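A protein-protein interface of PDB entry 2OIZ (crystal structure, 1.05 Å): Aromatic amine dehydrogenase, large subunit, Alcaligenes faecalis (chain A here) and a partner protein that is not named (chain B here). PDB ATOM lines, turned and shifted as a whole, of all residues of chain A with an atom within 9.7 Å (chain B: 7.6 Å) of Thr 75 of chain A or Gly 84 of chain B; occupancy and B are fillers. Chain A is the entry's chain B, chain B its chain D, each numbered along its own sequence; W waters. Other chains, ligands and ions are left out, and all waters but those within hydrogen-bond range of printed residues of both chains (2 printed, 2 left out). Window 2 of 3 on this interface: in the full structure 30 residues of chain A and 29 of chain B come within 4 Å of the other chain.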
ATOM      1  N   THR A  29       8.947 -36.612  15.707  1.00  0.00           N
ATOM      2  CA  THR A  29       8.296 -35.394  16.171  1.00  0.00           C
ATOM      3  C   THR A  29       7.259 -35.631  17.270  1.00  0.00           C
ATOM      4  O   THR A  29       6.748 -34.657  17.795  1.00  0.00           O
ATOM      5  CB  THR A  29       7.630 -34.583  15.042  1.00  0.00           C
ATOM      6  OG1 THR A  29       6.540 -35.334  14.516  1.00  0.00           O
ATOM      7  CG2 THR A  29       8.626 -34.157  13.978  1.00  0.00           C
ATOM      8  N   PHE A  51       9.902 -33.050  19.163  1.00  0.00           N
ATOM      9  CA  PHE A  51      10.950 -33.671  18.365  1.00  0.00           C
ATOM     10  C   PHE A  51      12.127 -34.077  19.234  1.00  0.00           C
ATOM     11  O   PHE A  51      12.795 -33.231  19.824  1.00  0.00           O
ATOM     12  CB  PHE A  51      11.428 -32.719  17.274  1.00  0.00           C
ATOM     13  CG  PHE A  51      12.523 -33.295  16.411  1.00  0.00           C
ATOM     14  CD1 PHE A  51      12.222 -34.218  15.412  1.00  0.00           C
ATOM     15  CD2 PHE A  51      13.845 -32.944  16.606  1.00  0.00           C
ATOM     16  CE1 PHE A  51      13.221 -34.750  14.615  1.00  0.00           C
ATOM     17  CE2 PHE A  51      14.846 -33.487  15.809  1.00  0.00           C
ATOM     18  CZ  PHE A  51      14.535 -34.375  14.790  1.00  0.00           C
ATOM     19  N   THR A  69      12.735 -29.529  20.854  1.00  0.00           N
ATOM     20  CA  THR A  69      12.720 -28.544  19.779  1.00  0.00           C
ATOM     21  C   THR A  69      11.318 -28.487  19.184  1.00  0.00           C
ATOM     22  O   THR A  69      10.748 -29.526  18.809  1.00  0.00           O
ATOM     23  CB  THR A  69      13.723 -28.921  18.669  1.00  0.00           C
ATOM     24  OG1 THR A  69      15.062 -28.914  19.197  1.00  0.00           O
ATOM     25  CG2 THR A  69      13.639 -28.024  17.455  1.00  0.00           C
ATOM     26  N   TYR A  70      10.831 -27.254  18.998  1.00  0.00           N
ATOM     27  CA  TYR A  70       9.625 -26.937  18.258  1.00  0.00           C
ATOM     28  C   TYR A  70       9.991 -26.112  17.032  1.00  0.00           C
ATOM     29  O   TYR A  70      11.003 -25.411  17.026  1.00  0.00           O
ATOM     30  CB  TYR A  70       8.667 -26.100  19.125  1.00  0.00           C
ATOM     31  CG  TYR A  70       8.184 -26.782  20.371  1.00  0.00           C
ATOM     32  CD1 TYR A  70       8.818 -26.585  21.579  1.00  0.00           C
ATOM     33  CD2 TYR A  70       7.096 -27.631  20.345  1.00  0.00           C
ATOM     34  CE1 TYR A  70       8.343 -27.166  22.738  1.00  0.00           C
ATOM     35  CE2 TYR A  70       6.635 -28.222  21.490  1.00  0.00           C
ATOM     36  CZ  TYR A  70       7.260 -27.989  22.692  1.00  0.00           C
ATOM     37  OH  TYR A  70       6.749 -28.584  23.867  1.00  0.00           O
ATOM     38  N   HIS A  71       9.129 -26.153  16.023  1.00  0.00           N
ATOM     39  CA  HIS A  71       9.117 -25.130  14.989  1.00  0.00           C
ATOM     40  C   HIS A  71       7.669 -24.652  14.801  1.00  0.00           C
ATOM     41  O   HIS A  71       6.732 -25.420  14.992  1.00  0.00           O
ATOM     42  CB  HIS A  71       9.683 -25.595  13.636  1.00  0.00           C
ATOM     43  CG  HIS A  71      11.098 -26.037  13.674  1.00  0.00           C
ATOM     44  ND1 HIS A  71      12.182 -25.301  13.226  1.00  0.00           N
ATOM     45  CD2 HIS A  71      11.591 -27.215  14.104  1.00  0.00           C
ATOM     46  CE1 HIS A  71      13.288 -26.024  13.394  1.00  0.00           C
ATOM     47  NE2 HIS A  71      12.945 -27.191  13.910  1.00  0.00           N
ATOM     48  N   GLU A  72       7.508 -23.418  14.331  1.00  0.00           N
ATOM     49  CA  GLU A  72       6.180 -22.831  14.211  1.00  0.00           C
ATOM     50  C   GLU A  72       5.231 -23.695  13.385  1.00  0.00           C
ATOM     51  O   GLU A  72       4.018 -23.754  13.651  1.00  0.00           O
ATOM     52  CB  GLU A  72       6.254 -21.458  13.573  1.00  0.00           C
ATOM     53  CG  GLU A  72       6.990 -20.360  14.301  1.00  0.00           C
ATOM     54  CD  GLU A  72       7.159 -19.048  13.434  1.00  0.00           C
ATOM     55  OE1 GLU A  72       7.755 -19.058  12.274  1.00  0.00           O
ATOM     56  OE2 GLU A  72       6.707 -17.982  13.933  1.00  0.00           O
ATOM     57  N   ARG A  73       5.768 -24.356  12.350  1.00  0.00           N
ATOM     58  CA  ARG A  73       4.970 -25.246  11.506  1.00  0.00           C
ATOM     59  C   ARG A  73       5.661 -26.612  11.347  1.00  0.00           C
ATOM     60  O   ARG A  73       5.501 -27.280  10.328  1.00  0.00           O
ATOM     61  CB  ARG A  73       4.732 -24.580  10.160  1.00  0.00           C
ATOM     62  CG  ARG A  73       3.864 -23.338  10.220  1.00  0.00           C
ATOM     63  CD  ARG A  73       2.390 -23.709  10.410  1.00  0.00           C
ATOM     64  NE  ARG A  73       1.482 -22.575  10.348  1.00  0.00           N
ATOM     65  CZ  ARG A  73       1.171 -21.802  11.370  1.00  0.00           C
ATOM     66  NH1 ARG A  73       1.638 -22.033  12.571  1.00  0.00           N
ATOM     67  NH2 ARG A  73       0.353 -20.776  11.167  1.00  0.00           N
ATOM     68  N   ILE A  74       6.379 -27.008  12.408  1.00  0.00           N
ATOM     69  CA  ILE A  74       6.998 -28.348  12.590  1.00  0.00           C
ATOM     70  C   ILE A  74       8.182 -28.549  11.645  1.00  0.00           C
ATOM     71  O   ILE A  74       9.345 -28.623  12.091  1.00  0.00           O
ATOM     72  CB  ILE A  74       5.994 -29.507  12.481  1.00  0.00           C
ATOM     73  CG1 ILE A  74       4.793 -29.294  13.415  1.00  0.00           C
ATOM     74  CG2 ILE A  74       6.710 -30.814  12.853  1.00  0.00           C
ATOM     75  CD1 ILE A  74       3.655 -30.164  13.174  1.00  0.00           C
ATOM     76  N   THR A  75       7.902 -28.673  10.355  1.00  0.00           N
ATOM     77  CA  THR A  75       8.888 -28.854   9.290  1.00  0.00           C
ATOM     78  C   THR A  75       9.299 -27.581   8.589  1.00  0.00           C
ATOM     79  O   THR A  75      10.140 -27.608   7.685  1.00  0.00           O
ATOM     80  CB  THR A  75       8.362 -29.881   8.278  1.00  0.00           C
ATOM     81  OG1 THR A  75       7.013 -29.557   7.935  1.00  0.00           O
ATOM     82  CG2 THR A  75       8.351 -31.275   8.894  1.00  0.00           C
ATOM     83  N   ARG A  76       8.741 -26.442   9.026  1.00  0.00           N
ATOM     84  CA  ARG A  76       9.158 -25.125   8.552  1.00  0.00           C
ATOM     85  C   ARG A  76       8.839 -24.122   9.685  1.00  0.00           C
ATOM     86  O   ARG A  76       8.159 -24.452  10.651  1.00  0.00           O
ATOM     87  CB  ARG A  76       8.475 -24.741   7.244  1.00  0.00           C
ATOM     88  CG  ARG A  76       6.969 -24.649   7.329  1.00  0.00           C
ATOM     89  CD  ARG A  76       6.264 -24.433   5.986  1.00  0.00           C
ATOM     90  NE  ARG A  76       4.813 -24.509   6.141  1.00  0.00           N
ATOM     91  CZ  ARG A  76       4.028 -23.512   6.522  1.00  0.00           C
ATOM     92  NH1 ARG A  76       4.538 -22.300   6.698  1.00  0.00           N
ATOM     93  NH2 ARG A  76       2.744 -23.752   6.744  1.00  0.00           N
ATOM     94  N   GLY A  77       9.314 -22.905   9.522  1.00  0.00           N
ATOM     95  CA  GLY A  77       9.121 -21.856  10.508  1.00  0.00           C
ATOM     96  C   GLY A  77      10.196 -21.801  11.568  1.00  0.00           C
ATOM     97  O   GLY A  77      11.109 -22.604  11.634  1.00  0.00           O
ATOM     98  N   LYS A  78      10.053 -20.816  12.443  1.00  0.00           N
ATOM     99  CA  LYS A  78      11.096 -20.507  13.412  1.00  0.00           C
ATOM    100  C   LYS A  78      11.254 -21.632  14.433  1.00  0.00           C
ATOM    101  O   LYS A  78      10.268 -22.194  14.908  1.00  0.00           O
ATOM    102  CB  LYS A  78      10.755 -19.224  14.157  1.00  0.00           C
ATOM    103  CG  LYS A  78      11.794 -18.808  15.175  1.00  0.00           C
ATOM    104  CD  LYS A  78      11.615 -17.392  15.677  1.00  0.00           C
ATOM    105  CE  LYS A  78      12.701 -16.980  16.688  1.00  0.00           C
ATOM    106  NZ  LYS A  78      14.056 -16.958  16.080  1.00  0.00           N
ATOM    107  N   ARG A  79      12.515 -21.933  14.745  1.00  0.00           N
ATOM    108  CA  ARG A  79      12.930 -22.934  15.723  1.00  0.00           C
ATOM    109  C   ARG A  79      12.867 -22.359  17.133  1.00  0.00           C
ATOM    110  O   ARG A  79      13.335 -21.240  17.380  1.00  0.00           O
ATOM    111  CB  ARG A  79      14.346 -23.389  15.431  1.00  0.00           C
ATOM    112  CG  ARG A  79      14.891 -24.453  16.366  1.00  0.00           C
ATOM    113  CD  ARG A  79      16.123 -25.084  15.801  1.00  0.00           C
ATOM    114  NE  ARG A  79      16.854 -25.907  16.757  1.00  0.00           N
ATOM    115  CZ  ARG A  79      17.949 -26.609  16.468  1.00  0.00           C
ATOM    116  NH1 ARG A  79      18.370 -26.703  15.204  1.00  0.00           N
ATOM    117  NH2 ARG A  79      18.589 -27.238  17.436  1.00  0.00           N
ATOM    118  N   GLN A 105      20.597 -32.600  19.367  1.00  0.00           N
ATOM    119  CA  GLN A 105      19.581 -33.505  18.814  1.00  0.00           C
ATOM    120  C   GLN A 105      20.313 -34.819  18.575  1.00  0.00           C
ATOM    121  O   GLN A 105      21.269 -34.892  17.803  1.00  0.00           O
ATOM    122  CB  GLN A 105      18.989 -32.916  17.545  1.00  0.00           C
ATOM    123  CG  GLN A 105      18.202 -31.632  17.848  1.00  0.00           C
ATOM    124  CD  GLN A 105      17.631 -30.960  16.644  1.00  0.00           C
ATOM    125  OE1 GLN A 105      16.714 -30.092  16.762  1.00  0.00           O
ATOM    126  NE2 GLN A 105      18.101 -31.306  15.497  1.00  0.00           N
ATOM    127  N   GLY B  54      11.596 -32.223  -2.039  1.00  0.00           N
ATOM    128  CA  GLY B  54      11.133 -31.395  -0.959  1.00  0.00           C
ATOM    129  C   GLY B  54      11.875 -31.571   0.345  1.00  0.00           C
ATOM    130  O   GLY B  54      11.464 -31.003   1.363  1.00  0.00           O
ATOM    131  N   SER B  55      12.961 -32.321   0.372  1.00  0.00           N
ATOM    132  CA  SER B  55      13.829 -32.425   1.521  1.00  0.00           C
ATOM    133  C   SER B  55      15.172 -31.809   1.184  1.00  0.00           C
ATOM    134  O   SER B  55      15.620 -31.812   0.037  1.00  0.00           O
ATOM    135  CB  SER B  55      13.967 -33.853   2.006  1.00  0.00           C
ATOM    136  OG  SER B  55      14.616 -34.696   1.089  1.00  0.00           O
ATOM    137  N   THR B  56      15.813 -31.213   2.181  1.00  0.00           N
ATOM    138  CA  THR B  56      16.942 -30.325   1.992  1.00  0.00           C
ATOM    139  C   THR B  56      18.250 -30.973   2.454  1.00  0.00           C
ATOM    140  O   THR B  56      18.279 -31.475   3.591  1.00  0.00           O
ATOM    141  CB  THR B  56      16.697 -28.997   2.839  1.00  0.00           C
ATOM    142  OG1 THR B  56      15.424 -28.436   2.446  1.00  0.00           O
ATOM    143  CG2 THR B  56      17.795 -27.992   2.664  1.00  0.00           C
ATOM    144  N   PRO B  57      19.319 -30.953   1.661  1.00  0.00           N
ATOM    145  CA  PRO B  57      20.570 -31.520   2.136  1.00  0.00           C
ATOM    146  C   PRO B  57      21.141 -30.831   3.349  1.00  0.00           C
ATOM    147  O   PRO B  57      21.032 -29.605   3.479  1.00  0.00           O
ATOM    148  CB  PRO B  57      21.521 -31.311   0.919  1.00  0.00           C
ATOM    149  CG  PRO B  57      20.636 -31.134  -0.250  1.00  0.00           C
ATOM    150  CD  PRO B  57      19.386 -30.495   0.257  1.00  0.00           C
ATOM    151  N   CYS B  82      19.105 -35.619   4.658  1.00  0.00           N
ATOM    152  CA  CYS B  82      18.085 -34.803   4.028  1.00  0.00           C
ATOM    153  C   CYS B  82      17.078 -34.453   5.128  1.00  0.00           C
ATOM    154  O   CYS B  82      16.731 -35.292   5.967  1.00  0.00           O
ATOM    155  CB  CYS B  82      17.417 -35.574   2.891  1.00  0.00           C
ATOM    156  SG  CYS B  82      18.582 -36.010   1.573  1.00  0.00           S
ATOM    157  N   CYS B  83      16.647 -33.208   5.116  1.00  0.00           N
ATOM    158  CA  CYS B  83      16.035 -32.565   6.267  1.00  0.00           C
ATOM    159  C   CYS B  83      14.777 -31.791   5.878  1.00  0.00           C
ATOM    160  O   CYS B  83      14.512 -31.482   4.724  1.00  0.00           O
ATOM    161  CB  CYS B  83      17.073 -31.583   6.838  1.00  0.00           C
ATOM    162  SG  CYS B  83      18.736 -32.314   7.095  1.00  0.00           S
ATOM    163  N   GLY B  84      13.983 -31.437   6.884  1.00  0.00           N
ATOM    164  CA  GLY B  84      12.826 -30.591   6.676  1.00  0.00           C
ATOM    165  C   GLY B  84      11.572 -31.319   6.245  1.00  0.00           C
ATOM    166  O   GLY B  84      10.617 -30.685   5.815  1.00  0.00           O
ATOM    167  N   LYS B  85      11.586 -32.643   6.354  1.00  0.00           N
ATOM    168  CA  LYS B  85      10.405 -33.475   6.228  1.00  0.00           C
ATOM    169  C   LYS B  85      10.504 -34.501   7.346  1.00  0.00           C
ATOM    170  O   LYS B  85      11.581 -34.825   7.828  1.00  0.00           O
ATOM    171  CB  LYS B  85      10.269 -34.181   4.883  1.00  0.00           C
ATOM    172  CG  LYS B  85       9.759 -33.272   3.796  1.00  0.00           C
ATOM    173  CD  LYS B  85       9.382 -33.981   2.498  1.00  0.00           C
ATOM    174  CE  LYS B  85       8.646 -33.022   1.646  1.00  0.00           C
ATOM    175  NZ  LYS B  85       8.379 -33.558   0.320  1.00  0.00           N
ATOM    176  N   THR B  86       9.339 -34.994   7.804  1.00  0.00           N
ATOM    177  CA  THR B  86       9.261 -35.983   8.866  1.00  0.00           C
ATOM    178  C   THR B  86       9.820 -37.355   8.394  1.00  0.00           C
ATOM    179  O   THR B  86      10.065 -37.593   7.197  1.00  0.00           O
ATOM    180  CB  THR B  86       7.856 -36.053   9.403  1.00  0.00           C
ATOM    181  OG1 THR B  86       6.957 -36.158   8.297  1.00  0.00           O
ATOM    182  CG2 THR B  86       7.531 -34.830  10.254  1.00  0.00           C
ATOM    183  N   ALA B  87      10.061 -38.218   9.363  1.00  0.00           N
ATOM    184  CA  ALA B  87      10.826 -39.426   9.162  1.00  0.00           C
ATOM    185  C   ALA B  87      10.324 -40.243   7.999  1.00  0.00           C
ATOM    186  O   ALA B  87       9.162 -40.616   7.940  1.00  0.00           O
ATOM    187  CB  ALA B  87      10.749 -40.261  10.422  1.00  0.00           C
ATOM    188  N   CYS B 114      21.148 -33.155  10.597  1.00  0.00           N
ATOM    189  CA  CYS B 114      20.295 -32.017  10.204  1.00  0.00           C
ATOM    190  C   CYS B 114      20.305 -30.858  11.225  1.00  0.00           C
ATOM    191  O   CYS B 114      19.608 -29.875  11.036  1.00  0.00           O
ATOM    192  CB  CYS B 114      18.834 -32.440  10.010  1.00  0.00           C
ATOM    193  SG  CYS B 114      18.477 -33.548   8.689  1.00  0.00           S
ATOM    194  N   ASN B 117      20.437 -27.247   9.942  1.00  0.00           N
ATOM    195  CA  ASN B 117      19.582 -26.858   8.839  1.00  0.00           C
ATOM    196  C   ASN B 117      18.532 -25.866   9.274  1.00  0.00           C
ATOM    197  O   ASN B 117      18.157 -25.777  10.424  1.00  0.00           O
ATOM    198  CB  ASN B 117      18.904 -28.094   8.217  1.00  0.00           C
ATOM    199  CG  ASN B 117      19.737 -28.748   7.138  1.00  0.00           C
ATOM    200  OD1 ASN B 117      19.282 -28.845   5.982  1.00  0.00           O
ATOM    201  ND2 ASN B 117      20.895 -29.244   7.483  1.00  0.00           N
ATOM    202  N   GLU B 118      17.992 -25.153   8.303  1.00  0.00           N
ATOM    203  CA  GLU B 118      16.910 -24.231   8.539  1.00  0.00           C
ATOM    204  C   GLU B 118      15.759 -24.932   9.238  1.00  0.00           C
ATOM    205  O   GLU B 118      15.103 -24.358  10.097  1.00  0.00           O
ATOM    206  CB  GLU B 118      16.471 -23.627   7.185  1.00  0.00           C
ATOM    207  CG  GLU B 118      15.399 -22.606   7.212  1.00  0.00           C
ATOM    208  CD  GLU B 118      15.458 -21.654   6.012  1.00  0.00           C
ATOM    209  OE1 GLU B 118      15.991 -22.015   4.898  1.00  0.00           O
ATOM    210  OE2 GLU B 118      14.960 -20.529   6.191  1.00  0.00           O
ATOM    211  N   ASN B 119      15.442 -26.152   8.808  1.00  0.00           N
ATOM    212  CA  ASN B 119      14.542 -27.038   9.540  1.00  0.00           C
ATOM    213  C   ASN B 119      15.276 -28.335   9.834  1.00  0.00           C
ATOM    214  O   ASN B 119      15.665 -29.064   8.925  1.00  0.00           O
ATOM    215  CB  ASN B 119      13.226 -27.320   8.839  1.00  0.00           C
ATOM    216  CG  ASN B 119      12.293 -28.029   9.766  1.00  0.00           C
ATOM    217  OD1 ASN B 119      12.261 -29.285   9.797  1.00  0.00           O
ATOM    218  ND2 ASN B 119      11.587 -27.258  10.609  1.00  0.00           N
ATOM    219  N   SER B 120      15.430 -28.620  11.125  1.00  0.00           N
ATOM    220  CA  SER B 120      16.229 -29.756  11.601  1.00  0.00           C
ATOM    221  C   SER B 120      15.471 -31.082  11.633  1.00  0.00           C
ATOM    222  O   SER B 120      16.061 -32.085  12.031  1.00  0.00           O
ATOM    223  CB  SER B 120      16.819 -29.435  12.977  1.00  0.00           C
ATOM    224  OG  SER B 120      15.820 -29.061  13.914  1.00  0.00           O
ATOM    225  N   THR B 121      14.215 -31.134  11.191  1.00  0.00           N
ATOM    226  CA  THR B 121      13.511 -32.407  11.229  1.00  0.00           C
ATOM    227  C   THR B 121      14.232 -33.389  10.292  1.00  0.00           C
ATOM    228  O   THR B 121      14.534 -33.078   9.142  1.00  0.00           O
ATOM    229  CB  THR B 121      12.059 -32.268  10.792  1.00  0.00           C
ATOM    230  OG1 THR B 121      11.417 -31.218  11.543  1.00  0.00           O
ATOM    231  CG2 THR B 121      11.256 -33.541  11.034  1.00  0.00           C
ATOM    232  N   PHE B 122      14.522 -34.574  10.815  1.00  0.00           N
ATOM    233  CA  PHE B 122      15.286 -35.588  10.075  1.00  0.00           C
ATOM    234  C   PHE B 122      14.382 -36.415   9.169  1.00  0.00           C
ATOM    235  O   PHE B 122      13.415 -37.025   9.627  1.00  0.00           O
ATOM    236  CB  PHE B 122      16.017 -36.491  11.071  1.00  0.00           C
ATOM    237  CG  PHE B 122      16.655 -37.693  10.412  1.00  0.00           C
ATOM    238  CD1 PHE B 122      17.750 -37.532   9.600  1.00  0.00           C
ATOM    239  CD2 PHE B 122      16.101 -38.932  10.520  1.00  0.00           C
ATOM    240  CE1 PHE B 122      18.330 -38.624   8.937  1.00  0.00           C
ATOM    241  CE2 PHE B 122      16.666 -40.034   9.876  1.00  0.00           C
ATOM    242  CZ  PHE B 122      17.759 -39.859   9.082  1.00  0.00           C
ATOM    243  N   HIS B 123      14.768 -36.483   7.892  1.00  0.00           N
ATOM    244  CA  HIS B 123      14.005 -37.236   6.913  1.00  0.00           C
ATOM    245  C   HIS B 123      14.677 -38.577   6.533  1.00  0.00           C
ATOM    246  O   HIS B 123      14.060 -39.649   6.650  1.00  0.00           O
ATOM    247  CB  HIS B 123      13.748 -36.372   5.667  1.00  0.00           C
ATOM    248  CG  HIS B 123      12.863 -37.047   4.658  1.00  0.00           C
ATOM    249  ND1 HIS B 123      11.627 -37.563   4.974  1.00  0.00           N
ATOM    250  CD2 HIS B 123      13.030 -37.268   3.333  1.00  0.00           C
ATOM    251  CE1 HIS B 123      11.090 -38.075   3.872  1.00  0.00           C
ATOM    252  NE2 HIS B 123      11.934 -37.934   2.865  1.00  0.00           N
ATOM    253  N   CYS B 124      15.908 -38.502   6.037  1.00  0.00           N
ATOM    254  CA  CYS B 124      16.671 -39.693   5.614  1.00  0.00           C
ATOM    255  C   CYS B 124      18.152 -39.349   5.542  1.00  0.00           C
ATOM    256  O   CYS B 124      18.527 -38.189   5.647  1.00  0.00           O
ATOM    257  CB  CYS B 124      16.126 -40.285   4.307  1.00  0.00           C
ATOM    258  SG  CYS B 124      16.268 -39.192   2.872  1.00  0.00           S
HETATM  259  O   HOH W   1      11.014 -27.640   5.045  1.00  0.00           O
HETATM  260  O   HOH W   2      12.248 -24.455   9.988  1.00  0.00           O
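Of the 14 printed residues of chain A, 8 touch a printed residue of chain B.
Hydrophobic or aromatic side chains of chain A that line the printed part of chain B: Phe 51 and His 71.
Of the 19 printed residues of chain B, 6 touch a printed residue of chain A.
Among the printed residues, 14 pairs touch across the chains.
Water W2 lies within hydrogen-bond range of the backbone carbonyl oxygen (O) of Gly 77 of chain A (2.7 Å), the backbone carbonyl oxygen (O) of Glu 118 of chain B (2.9 Å), the side-chain amide nitrogen (ND2) of Asn 119 of chain B (2.9 Å) and a ring nitrogen (ND1) of His 71 of chain A (3.3 Å).
Water W1 bridges the backbone carbonyl oxygen (O) of Thr 75 of chain A and the backbone carbonyl oxygen (O) of Gly 84 of chain B.
The backbone NH (N) of Gly 84 of chain B lies within hydrogen-bond range of the backbone carbonyl oxygen (O) of Thr 121 of chain B, at 2.8 Å.
ND1 of His 123 of chain B lies within hydrogen-bond range of O of Thr 86 of chain B (2.7 Å).
OD1 of Asn 119 of chain B sits at hydrogen-bond distance from OG1 of Thr 121 of chain B, at 2.7 Å.
OG1 of Thr 69 of chain A is in hydrogen-bond range of OE1 of Gln 105 of chain A (3.2 Å).
The side-chain amide oxygen of Gln 105 of chain A sits at hydrogen-bond distance from the guanidinium group of Arg 79 of chain A (3.5 Å).
SG of Cys 114 of chain B forms a disulfide with SG of Cys 83 of chain B.
Among the printed residues, merely in contact across the chains: Thr 29 of chain A with Thr 86 of chain B, Thr 29 of chain A with Thr 121 of chain B, Phe 51 of chain A with Ser 120 of chain B, Phe 51 of chain A with Phe 122 of chain B, Thr 75 of chain A with Gly 84 of chain B, Thr 75 of chain A with Thr 86 of chain B and Arg 79 of chain A with Ser 120 of chain B.
Of the printed residues of chain B, Thr 75 of chain A touches Gly 84, Thr 86 and Asn 119.
No residue of chain A comes within 4 Å of Cys 83 of chain B.
Asn 119 of chain B touches four residues of chain A.
Printed residues of chain B within 4 Å of Thr 29 of chain A: Thr 86 (3.9 Å) and Thr 121 (3.995 Å).
Printed residues of chain B within 4 Å of Gln 105 of chain A: Ser 120 (3.2 Å).
Of the printed residues of chain A, Thr 86 of chain B touches Thr 29 (3.9 Å) and Thr 75 (3.9 Å).
Of the printed residues of chain B, His 71 of chain A touches Asn 119 (3.3 Å) and Ser 120 (3.4 Å).
Of the printed residues of chain A, Phe 122 of chain B touches Phe 51.
Cys 114 of chain B touches none of the printed residues of chain A.
The nearest residue of chain A that does not touch Gly 84 of chain B is Arg 76 of chain A (5.6 Å).
The nearest printed residue of chain B that does not touch Thr 29 of chain A is Ala 87 of chain B (6.3 Å).
ND2 of Asn 119 of chain B lies within hydrogen-bond range of ND1 of His 71 of chain A.
ND2 of Asn 119 of chain B sits at hydrogen-bond distance from O of Ile 74 of chain A (3.0 Å).
The side-chain amide nitrogen (ND2) of Asn 119 of chain B sits close to the backbone carbonyl oxygen (O) of Thr 75 of chain A (3.3 Å).
N of Arg 76 of chain A sits close to ND2 of Asn 119 of chain B (3.4 Å).
A ring nitrogen (NE2) of His 71 of chain A sits at hydrogen-bond distance from the side-chain hydroxyl (OG) of Ser 120 of chain B, at 3.4 Å.
The side-chain hydroxyl of Ser 120 of chain B is in hydrogen-bond range of the side-chain amide oxygen of Gln 105 of chain A (3.2 Å).
O of Ile 74 of chain A sits at hydrogen-bond distance from OG1 of Thr 121 of chain B (3.4 Å).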
